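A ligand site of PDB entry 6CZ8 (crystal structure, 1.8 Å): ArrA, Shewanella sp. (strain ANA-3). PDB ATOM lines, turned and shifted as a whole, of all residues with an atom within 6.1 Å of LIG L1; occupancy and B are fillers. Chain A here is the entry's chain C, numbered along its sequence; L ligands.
A sulfur (S2) of LIG L1 lies close to the backbone NH (N) of Cys 24. The side-chain sulfur (SG) of Cys 56 binds an iron atom (FE2) of LIG L1 (2.3 Å). A nitrogen (N10) of LG2 L2 lies close to the side-chain sulfur (SG) of Cys 24 (3.7 Å). The side-chain amide nitrogen (ND2) of Asn 192 sits at hydrogen-bond distance from an oxygen (O6) of LG2 L2. A sulfur (S4) of LIG L1 lies close to the side-chain hydroxyl (OG) of Ser 196 (3.7 Å). The side-chain amino group (NZ) of Lys 30 sits close to a sulfur (S1) of LIG L1 (3.2 Å). SG of Cys 24 binds FE1 of LIG L1, at 2.4 Å. An oxygen (O12) of LG2 L2 lies within hydrogen-bond range of the backbone NH (N) of Asn 192, at 3.2 Å. The side-chain hydroxyl of Ser 26 sits close to a sulfur (S4) of LIG L1 (3.6 Å). N of Cys 28 sits close to S2 of LIG L1, at 3.5 Å. A nitrogen (N9) of LG2 L2 lies within hydrogen-bond range of the guanidinium group of Arg 58, 3.4 Å away. The backbone carbonyl oxygen (O) of Asn 192 is in hydrogen-bond range of a nitrogen (N10) of LG2 L2, 2.7 Å away. The backbone carbonyl oxygen (O) of Asn 688 is in hydrogen-bond range of a nitrogen (N7) of LG2 L2 (2.7 Å). SG of Cys 21 is bound to FE4 of LIG L1. The side-chain hydroxyl (OG) of Ser 55 sits close to a sulfur (S1) of LIG L1. An iron atom (FE3) of LIG L1 is bound by the side-chain sulfur of Cys 28 (2.3 Å). A sulfur (S2) of LIG L1 lies close to the backbone NH (N) of Trp 27, at 3.5 Å. NH1 of Arg 58 sits close to S3 of LIG L1, at 3.5 Å.
The side-chain amide nitrogen (NE2) of Gln 194 sits close to the side-chain sulfur (SG) of Cys 28 (3.6 Å). NH1 of Arg 58 is in hydrogen-bond range of O of Asn 688 (3.0 Å). NE1 of Trp 27 sits close to NE2 of Gln 22 (3.4 Å). The guanidinium group (NE) of Arg 58 lies close to the side-chain sulfur (SG) of Cys 56 (3.3 Å). The backbone NH (N) of Cys 21 is in hydrogen-bond range of the backbone carbonyl oxygen (O) of Cys 28, at 2.9 Å. NH2 of Arg 58 lies close to SG of Cys 24 (3.3 Å). The backbone NH (N) of Gly 23 lies close to the side-chain sulfur (SG) of Cys 21 (3.5 Å). The side-chain hydroxyl of Ser 26 sits at hydrogen-bond distance from the backbone NH of Val 195 (3.1 Å).
Gly 23 touches LIG L1. Val 195 touches LIG L1. Hydrophobic or aromatic side chains that line LIG L1: Val 195. Along chain A the residues within 4 Å of LIG L1 span positions 21 to 196.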
ATOM      1  N   CYS A  21      -6.551  28.252 -10.048  1.00  0.00           N
ATOM      2  CA  CYS A  21      -7.174  27.340 -10.996  1.00  0.00           C
ATOM      3  C   CYS A  21      -7.562  26.042 -10.310  1.00  0.00           C
ATOM      4  O   CYS A  21      -6.907  25.593  -9.358  1.00  0.00           O
ATOM      5  CB  CYS A  21      -6.201  27.088 -12.156  1.00  0.00           C
ATOM      6  SG  CYS A  21      -6.860  26.098 -13.581  1.00  0.00           S
ATOM      7  N   GLN A  22      -8.656  25.432 -10.792  1.00  0.00           N
ATOM      8  CA  GLN A  22      -9.052  24.114 -10.287  1.00  0.00           C
ATOM      9  C   GLN A  22      -9.368  23.127 -11.408  1.00  0.00           C
ATOM     10  O   GLN A  22     -10.128  22.168 -11.218  1.00  0.00           O
ATOM     11  CB  GLN A  22     -10.221  24.208  -9.312  1.00  0.00           C
ATOM     12  CG  GLN A  22      -9.858  24.981  -8.026  1.00  0.00           C
ATOM     13  CD  GLN A  22     -10.925  24.896  -6.975  1.00  0.00           C
ATOM     14  OE1 GLN A  22     -11.791  25.758  -6.858  1.00  0.00           O
ATOM     15  NE2 GLN A  22     -10.884  23.814  -6.224  1.00  0.00           N
ATOM     16  N   GLY A  23      -8.720  23.300 -12.561  1.00  0.00           N
ATOM     17  CA  GLY A  23      -8.836  22.305 -13.611  1.00  0.00           C
ATOM     18  C   GLY A  23      -8.356  20.919 -13.222  1.00  0.00           C
ATOM     19  O   GLY A  23      -8.738  19.927 -13.865  1.00  0.00           O
ATOM     20  N   CYS A  24      -7.514  20.834 -12.206  1.00  0.00           N
ATOM     21  CA  CYS A  24      -7.208  19.575 -11.556  1.00  0.00           C
ATOM     22  C   CYS A  24      -6.743  19.895 -10.136  1.00  0.00           C
ATOM     23  O   CYS A  24      -6.603  21.071  -9.774  1.00  0.00           O
ATOM     24  CB  CYS A  24      -6.170  18.763 -12.330  1.00  0.00           C
ATOM     25  SG  CYS A  24      -4.580  19.582 -12.560  1.00  0.00           S
ATOM     26  N   THR A  25      -6.508  18.863  -9.354  1.00  0.00           N
ATOM     27  CA  THR A  25      -6.114  19.022  -7.953  1.00  0.00           C
ATOM     28  C   THR A  25      -4.653  19.450  -7.800  1.00  0.00           C
ATOM     29  O   THR A  25      -4.130  19.491  -6.669  1.00  0.00           O
ATOM     30  CB  THR A  25      -6.397  17.718  -7.194  1.00  0.00           C
ATOM     31  OG1 THR A  25      -5.888  16.605  -7.942  1.00  0.00           O
ATOM     32  CG2 THR A  25      -7.899  17.543  -6.999  1.00  0.00           C
ATOM     33  N   SER A  26      -3.985  19.823  -8.893  1.00  0.00           N
ATOM     34  CA  SER A  26      -2.779  20.632  -8.791  1.00  0.00           C
ATOM     35  C   SER A  26      -3.099  21.965  -8.122  1.00  0.00           C
ATOM     36  O   SER A  26      -2.259  22.508  -7.395  1.00  0.00           O
ATOM     37  CB  SER A  26      -2.171  20.861 -10.183  1.00  0.00           C
ATOM     38  OG  SER A  26      -1.852  19.614 -10.835  1.00  0.00           O
ATOM     39  N   TRP A  27      -4.285  22.506  -8.381  1.00  0.00           N
ATOM     40  CA  TRP A  27      -4.765  23.757  -7.769  1.00  0.00           C
ATOM     41  C   TRP A  27      -3.719  24.886  -7.845  1.00  0.00           C
ATOM     42  O   TRP A  27      -3.316  25.481  -6.841  1.00  0.00           O
ATOM     43  CB  TRP A  27      -5.200  23.484  -6.328  1.00  0.00           C
ATOM     44  CG  TRP A  27      -6.450  22.642  -6.211  1.00  0.00           C
ATOM     45  CD1 TRP A  27      -7.376  22.403  -7.187  1.00  0.00           C
ATOM     46  CD2 TRP A  27      -6.897  21.927  -5.056  1.00  0.00           C
ATOM     47  NE1 TRP A  27      -8.386  21.593  -6.703  1.00  0.00           N
ATOM     48  CE2 TRP A  27      -8.107  21.284  -5.393  1.00  0.00           C
ATOM     49  CE3 TRP A  27      -6.402  21.786  -3.752  1.00  0.00           C
ATOM     50  CZ2 TRP A  27      -8.802  20.493  -4.486  1.00  0.00           C
ATOM     51  CZ3 TRP A  27      -7.087  20.979  -2.867  1.00  0.00           C
ATOM     52  CH2 TRP A  27      -8.280  20.351  -3.226  1.00  0.00           C
ATOM     53  N   CYS A  28      -3.324  25.192  -9.080  1.00  0.00           N
ATOM     54  CA  CYS A  28      -2.252  26.151  -9.278  1.00  0.00           C
ATOM     55  C   CYS A  28      -2.676  27.582  -8.951  1.00  0.00           C
ATOM     56  O   CYS A  28      -3.769  28.037  -9.318  1.00  0.00           O
ATOM     57  CB  CYS A  28      -1.763  26.138 -10.723  1.00  0.00           C
ATOM     58  SG  CYS A  28      -1.140  24.569 -11.330  1.00  0.00           S
ATOM     59  N   LYS A  30      -2.674  31.365  -9.778  1.00  0.00           N
ATOM     60  CA  LYS A  30      -2.743  32.044 -11.058  1.00  0.00           C
ATOM     61  C   LYS A  30      -2.791  33.558 -10.893  1.00  0.00           C
ATOM     62  O   LYS A  30      -3.133  34.083  -9.822  1.00  0.00           O
ATOM     63  CB  LYS A  30      -4.029  31.627 -11.844  1.00  0.00           C
ATOM     64  CG  LYS A  30      -4.073  30.154 -12.212  1.00  0.00           C
ATOM     65  CD  LYS A  30      -2.887  29.776 -13.064  1.00  0.00           C
ATOM     66  CE  LYS A  30      -3.059  28.464 -13.728  1.00  0.00           C
ATOM     67  NZ  LYS A  30      -1.879  28.127 -14.558  1.00  0.00           N
ATOM     68  N   SER A  55       2.772  26.626 -16.240  1.00  0.00           N
ATOM     69  CA  SER A  55       1.388  26.184 -16.317  1.00  0.00           C
ATOM     70  C   SER A  55       1.209  25.074 -17.360  1.00  0.00           C
ATOM     71  O   SER A  55       1.894  25.024 -18.374  1.00  0.00           O
ATOM     72  CB  SER A  55       0.464  27.341 -16.737  1.00  0.00           C
ATOM     73  OG  SER A  55      -0.882  26.895 -16.783  1.00  0.00           O
ATOM     74  N   CYS A  56       0.244  24.205 -17.098  1.00  0.00           N
ATOM     75  CA  CYS A  56      -0.292  23.301 -18.127  1.00  0.00           C
ATOM     76  C   CYS A  56      -1.201  24.066 -19.085  1.00  0.00           C
ATOM     77  O   CYS A  56      -1.509  25.246 -18.888  1.00  0.00           O
ATOM     78  CB  CYS A  56      -1.057  22.164 -17.438  1.00  0.00           C
ATOM     79  SG  CYS A  56      -2.871  22.283 -17.366  1.00  0.00           S
ATOM     80  N   PRO A  57      -1.614  23.445 -20.189  1.00  0.00           N
ATOM     81  CA  PRO A  57      -2.325  24.204 -21.234  1.00  0.00           C
ATOM     82  C   PRO A  57      -3.742  24.579 -20.875  1.00  0.00           C
ATOM     83  O   PRO A  57      -4.293  25.480 -21.523  1.00  0.00           O
ATOM     84  CB  PRO A  57      -2.299  23.251 -22.454  1.00  0.00           C
ATOM     85  CG  PRO A  57      -2.261  21.863 -21.825  1.00  0.00           C
ATOM     86  CD  PRO A  57      -1.379  22.032 -20.561  1.00  0.00           C
ATOM     87  N   ARG A  58      -4.361  23.887 -19.896  1.00  0.00           N
ATOM     88  CA  ARG A  58      -5.777  24.097 -19.606  1.00  0.00           C
ATOM     89  C   ARG A  58      -6.034  25.442 -18.966  1.00  0.00           C
ATOM     90  O   ARG A  58      -7.187  25.868 -18.940  1.00  0.00           O
ATOM     91  CB  ARG A  58      -6.310  22.966 -18.716  1.00  0.00           C
ATOM     92  CG  ARG A  58      -6.392  21.623 -19.439  1.00  0.00           C
ATOM     93  CD  ARG A  58      -6.598  20.476 -18.480  1.00  0.00           C
ATOM     94  NE  ARG A  58      -5.387  20.206 -17.704  1.00  0.00           N
ATOM     95  CZ  ARG A  58      -5.352  19.710 -16.472  1.00  0.00           C
ATOM     96  NH1 ARG A  58      -6.468  19.420 -15.840  1.00  0.00           N
ATOM     97  NH2 ARG A  58      -4.170  19.535 -15.874  1.00  0.00           N
ATOM     98  N   GLN A  59      -5.009  26.151 -18.490  1.00  0.00           N
ATOM     99  CA  GLN A  59      -5.276  27.450 -17.876  1.00  0.00           C
ATOM    100  C   GLN A  59      -6.030  28.364 -18.843  1.00  0.00           C
ATOM    101  O   GLN A  59      -6.900  29.139 -18.426  1.00  0.00           O
ATOM    102  CB  GLN A  59      -3.980  28.116 -17.412  1.00  0.00           C
ATOM    103  CG  GLN A  59      -3.028  28.548 -18.478  1.00  0.00           C
ATOM    104  CD  GLN A  59      -1.842  29.349 -17.904  1.00  0.00           C
ATOM    105  OE1 GLN A  59      -1.913  29.868 -16.779  1.00  0.00           O
ATOM    106  NE2 GLN A  59      -0.762  29.450 -18.662  1.00  0.00           N
ATOM    107  N   SER A  62      -9.931  28.119 -19.231  1.00  0.00           N
ATOM    108  CA  SER A  62     -10.709  28.779 -18.193  1.00  0.00           C
ATOM    109  C   SER A  62     -11.548  29.920 -18.765  1.00  0.00           C
ATOM    110  O   SER A  62     -12.643  30.201 -18.275  1.00  0.00           O
ATOM    111  CB  SER A  62      -9.758  29.343 -17.111  1.00  0.00           C
ATOM    112  OG  SER A  62      -8.849  28.366 -16.678  1.00  0.00           O
ATOM    113  N   ASN A 192      -2.305  13.878 -13.158  1.00  0.00           N
ATOM    114  CA  ASN A 192      -1.778  13.865 -11.797  1.00  0.00           C
ATOM    115  C   ASN A 192      -1.778  15.283 -11.203  1.00  0.00           C
ATOM    116  O   ASN A 192      -2.478  16.173 -11.700  1.00  0.00           O
ATOM    117  CB  ASN A 192      -0.388  13.209 -11.748  1.00  0.00           C
ATOM    118  CG  ASN A 192      -0.095  12.522 -10.396  1.00  0.00           C
ATOM    119  OD1 ASN A 192       0.340  13.161  -9.442  1.00  0.00           O
ATOM    120  ND2 ASN A 192      -0.329  11.222 -10.342  1.00  0.00           N
ATOM    121  N   GLN A 194       0.534  17.852 -10.062  1.00  0.00           N
ATOM    122  CA  GLN A 194       1.149  19.158 -10.300  1.00  0.00           C
ATOM    123  C   GLN A 194       1.589  19.219 -11.751  1.00  0.00           C
ATOM    124  O   GLN A 194       2.785  19.174 -12.056  1.00  0.00           O
ATOM    125  CB  GLN A 194       2.312  19.413  -9.332  1.00  0.00           C
ATOM    126  CG  GLN A 194       2.150  20.764  -8.586  1.00  0.00           C
ATOM    127  CD  GLN A 194       1.744  21.937  -9.494  1.00  0.00           C
ATOM    128  OE1 GLN A 194       2.124  21.980 -10.668  1.00  0.00           O
ATOM    129  NE2 GLN A 194       0.936  22.836  -8.974  1.00  0.00           N
ATOM    130  N   VAL A 195       0.617  19.281 -12.663  1.00  0.00           N
ATOM    131  CA  VAL A 195       0.960  19.181 -14.067  1.00  0.00           C
ATOM    132  C   VAL A 195       1.892  20.329 -14.455  1.00  0.00           C
ATOM    133  O   VAL A 195       2.823  20.132 -15.235  1.00  0.00           O
ATOM    134  CB  VAL A 195      -0.314  19.135 -14.927  1.00  0.00           C
ATOM    135  CG1 VAL A 195       0.054  18.902 -16.386  1.00  0.00           C
ATOM    136  CG2 VAL A 195      -1.248  18.036 -14.454  1.00  0.00           C
ATOM    137  N   SER A 196       1.677  21.514 -13.879  1.00  0.00           N
ATOM    138  CA  SER A 196       2.511  22.661 -14.205  1.00  0.00           C
ATOM    139  C   SER A 196       3.970  22.427 -13.807  1.00  0.00           C
ATOM    140  O   SER A 196       4.888  22.622 -14.601  1.00  0.00           O
ATOM    141  CB  SER A 196       1.948  23.912 -13.516  1.00  0.00           C
ATOM    142  OG  SER A 196       0.605  24.141 -13.924  1.00  0.00           O
ATOM    143  N   ASN A 688      -8.849  18.070 -20.440  1.00  0.00           N
ATOM    144  CA  ASN A 688      -9.973  17.985 -19.513  1.00  0.00           C
ATOM    145  C   ASN A 688      -9.670  18.808 -18.266  1.00  0.00           C
ATOM    146  O   ASN A 688      -8.721  18.480 -17.536  1.00  0.00           O
ATOM    147  CB  ASN A 688     -10.237  16.560 -19.024  1.00  0.00           C
ATOM    148  CG  ASN A 688     -11.053  15.737 -19.960  1.00  0.00           C
ATOM    149  OD1 ASN A 688     -11.590  16.200 -20.973  1.00  0.00           O
ATOM    150  ND2 ASN A 688     -11.152  14.473 -19.611  1.00  0.00           N
ATOM    151  N   LYS A 689     -10.495  19.813 -17.965  1.00  0.00           N
ATOM    152  CA  LYS A 689     -10.562  20.390 -16.615  1.00  0.00           C
ATOM    153  C   LYS A 689     -11.623  19.562 -15.868  1.00  0.00           C
ATOM    154  O   LYS A 689     -12.797  19.936 -15.772  1.00  0.00           O
ATOM    155  CB  LYS A 689     -10.879  21.878 -16.652  1.00  0.00           C
ATOM    156  CG  LYS A 689      -9.737  22.727 -17.279  1.00  0.00           C
ATOM    157  CD  LYS A 689      -9.985  24.211 -17.184  1.00  0.00           C
ATOM    158  CE  LYS A 689      -9.635  24.724 -15.761  1.00  0.00           C
ATOM    159  NZ  LYS A 689     -10.090  26.183 -15.577  1.00  0.00           N
HETATM  160 FE1  LIG L   1      -4.655  21.875 -13.174  1.00  0.00          FE
HETATM  161 FE2  LIG L   1      -3.440  23.077 -15.275  1.00  0.00          FE
HETATM  162 FE3  LIG L   1      -2.835  23.844 -12.765  1.00  0.00          FE
HETATM  163 FE4  LIG L   1      -5.257  24.469 -13.795  1.00  0.00          FE
HETATM  164  S1  LIG L   1      -3.201  25.215 -14.610  1.00  0.00           S
HETATM  165  S2  LIG L   1      -4.893  23.524 -11.687  1.00  0.00           S
HETATM  166  S3  LIG L   1      -5.697  22.694 -15.042  1.00  0.00           S
HETATM  167  S4  LIG L   1      -2.354  21.854 -13.659  1.00  0.00           S
HETATM  168  P1  LG2 L   2      -5.214   9.489 -14.402  1.00  0.00           P
HETATM  169  O1  LG2 L   2      -4.937  10.889 -14.854  1.00  0.00           O
HETATM  170  O2  LG2 L   2      -6.587   9.321 -13.901  1.00  0.00           O
HETATM  171  O3  LG2 L   2      -4.180   9.111 -13.194  1.00  0.00           O
HETATM  172  O4  LG2 L   2      -4.143  11.419 -11.755  1.00  0.00           O
HETATM  173  P2  LG2 L   2      -3.569   9.909 -11.889  1.00  0.00           P
HETATM  174  O5  LG2 L   2      -3.919   9.055 -10.703  1.00  0.00           O
HETATM  175  O6  LG2 L   2      -2.102   9.975 -12.157  1.00  0.00           O
HETATM  176  O7  LG2 L   2      -4.875   8.471 -15.655  1.00  0.00           O
HETATM  177  C1  LG2 L   2      -4.956   7.097 -15.558  1.00  0.00           C
HETATM  178  C2  LG2 L   2      -3.821   6.534 -16.429  1.00  0.00           C
HETATM  179  O8  LG2 L   2      -3.794   4.970 -16.108  1.00  0.00           O
HETATM  180  C3  LG2 L   2      -4.001   6.586 -17.737  1.00  0.00           C
HETATM  181  O9  LG2 L   2      -2.683   6.994 -18.342  1.00  0.00           O
HETATM  182  C4  LG2 L   2      -4.400   5.226 -18.352  1.00  0.00           C
HETATM  183  O10 LG2 L   2      -3.773   4.911 -19.536  1.00  0.00           O
HETATM  184  C5  LG2 L   2      -3.728   4.338 -17.328  1.00  0.00           C
HETATM  185  N1  LG2 L   2      -3.991   2.946 -16.962  1.00  0.00           N
HETATM  186  C6  LG2 L   2      -5.246   2.652 -17.263  1.00  0.00           C
HETATM  187  N2  LG2 L   2      -5.401   1.328 -16.872  1.00  0.00           N
HETATM  188  C7  LG2 L   2      -4.231   0.922 -16.316  1.00  0.00           C
HETATM  189  C8  LG2 L   2      -3.659  -0.334 -15.669  1.00  0.00           C
HETATM  190  O11 LG2 L   2      -4.292  -1.327 -15.529  1.00  0.00           O
HETATM  191  N3  LG2 L   2      -2.302  -0.327 -15.233  1.00  0.00           N
HETATM  192  C9  LG2 L   2      -1.474   0.832 -15.359  1.00  0.00           C
HETATM  193  N4  LG2 L   2      -0.091   0.919 -15.005  1.00  0.00           N
HETATM  194  N5  LG2 L   2      -1.992   2.010 -15.956  1.00  0.00           N
HETATM  195  C10 LG2 L   2      -3.393   1.973 -16.398  1.00  0.00           C
HETATM  196  C11 LG2 L   2      -5.438  11.616 -11.203  1.00  0.00           C
HETATM  197  C12 LG2 L   2      -5.585  13.030 -10.742  1.00  0.00           C
HETATM  198  O12 LG2 L   2      -5.290  13.994 -11.967  1.00  0.00           O
HETATM  199  C13 LG2 L   2      -6.839  13.303 -10.311  1.00  0.00           C
HETATM  200  S1  LG2 L   2      -7.557  12.282  -9.016  1.00  0.00           S
HETATM  201  C14 LG2 L   2      -7.476  14.650 -10.558  1.00  0.00           C
HETATM  202  S2  LG2 L   2      -9.062  14.986  -9.840  1.00  0.00           S
HETATM  203  C15 LG2 L   2      -6.969  15.580 -11.539  1.00  0.00           C
HETATM  204  N6  LG2 L   2      -7.840  15.383 -12.775  1.00  0.00           N
HETATM  205  C16 LG2 L   2      -7.267  15.782 -13.963  1.00  0.00           C
HETATM  206  C17 LG2 L   2      -8.118  15.998 -15.166  1.00  0.00           C
HETATM  207  O13 LG2 L   2      -9.297  15.886 -15.152  1.00  0.00           O
HETATM  208  N7  LG2 L   2      -7.444  16.358 -16.392  1.00  0.00           N
HETATM  209  C18 LG2 L   2      -5.976  16.492 -16.559  1.00  0.00           C
HETATM  210  N8  LG2 L   2      -5.378  16.854 -17.812  1.00  0.00           N
HETATM  211  N9  LG2 L   2      -5.124  16.340 -15.378  1.00  0.00           N
HETATM  212  C19 LG2 L   2      -5.710  15.975 -14.118  1.00  0.00           C
HETATM  213  N10 LG2 L   2      -4.860  15.884 -13.035  1.00  0.00           N
HETATM  214  C20 LG2 L   2      -5.564  15.356 -11.775  1.00  0.00           C
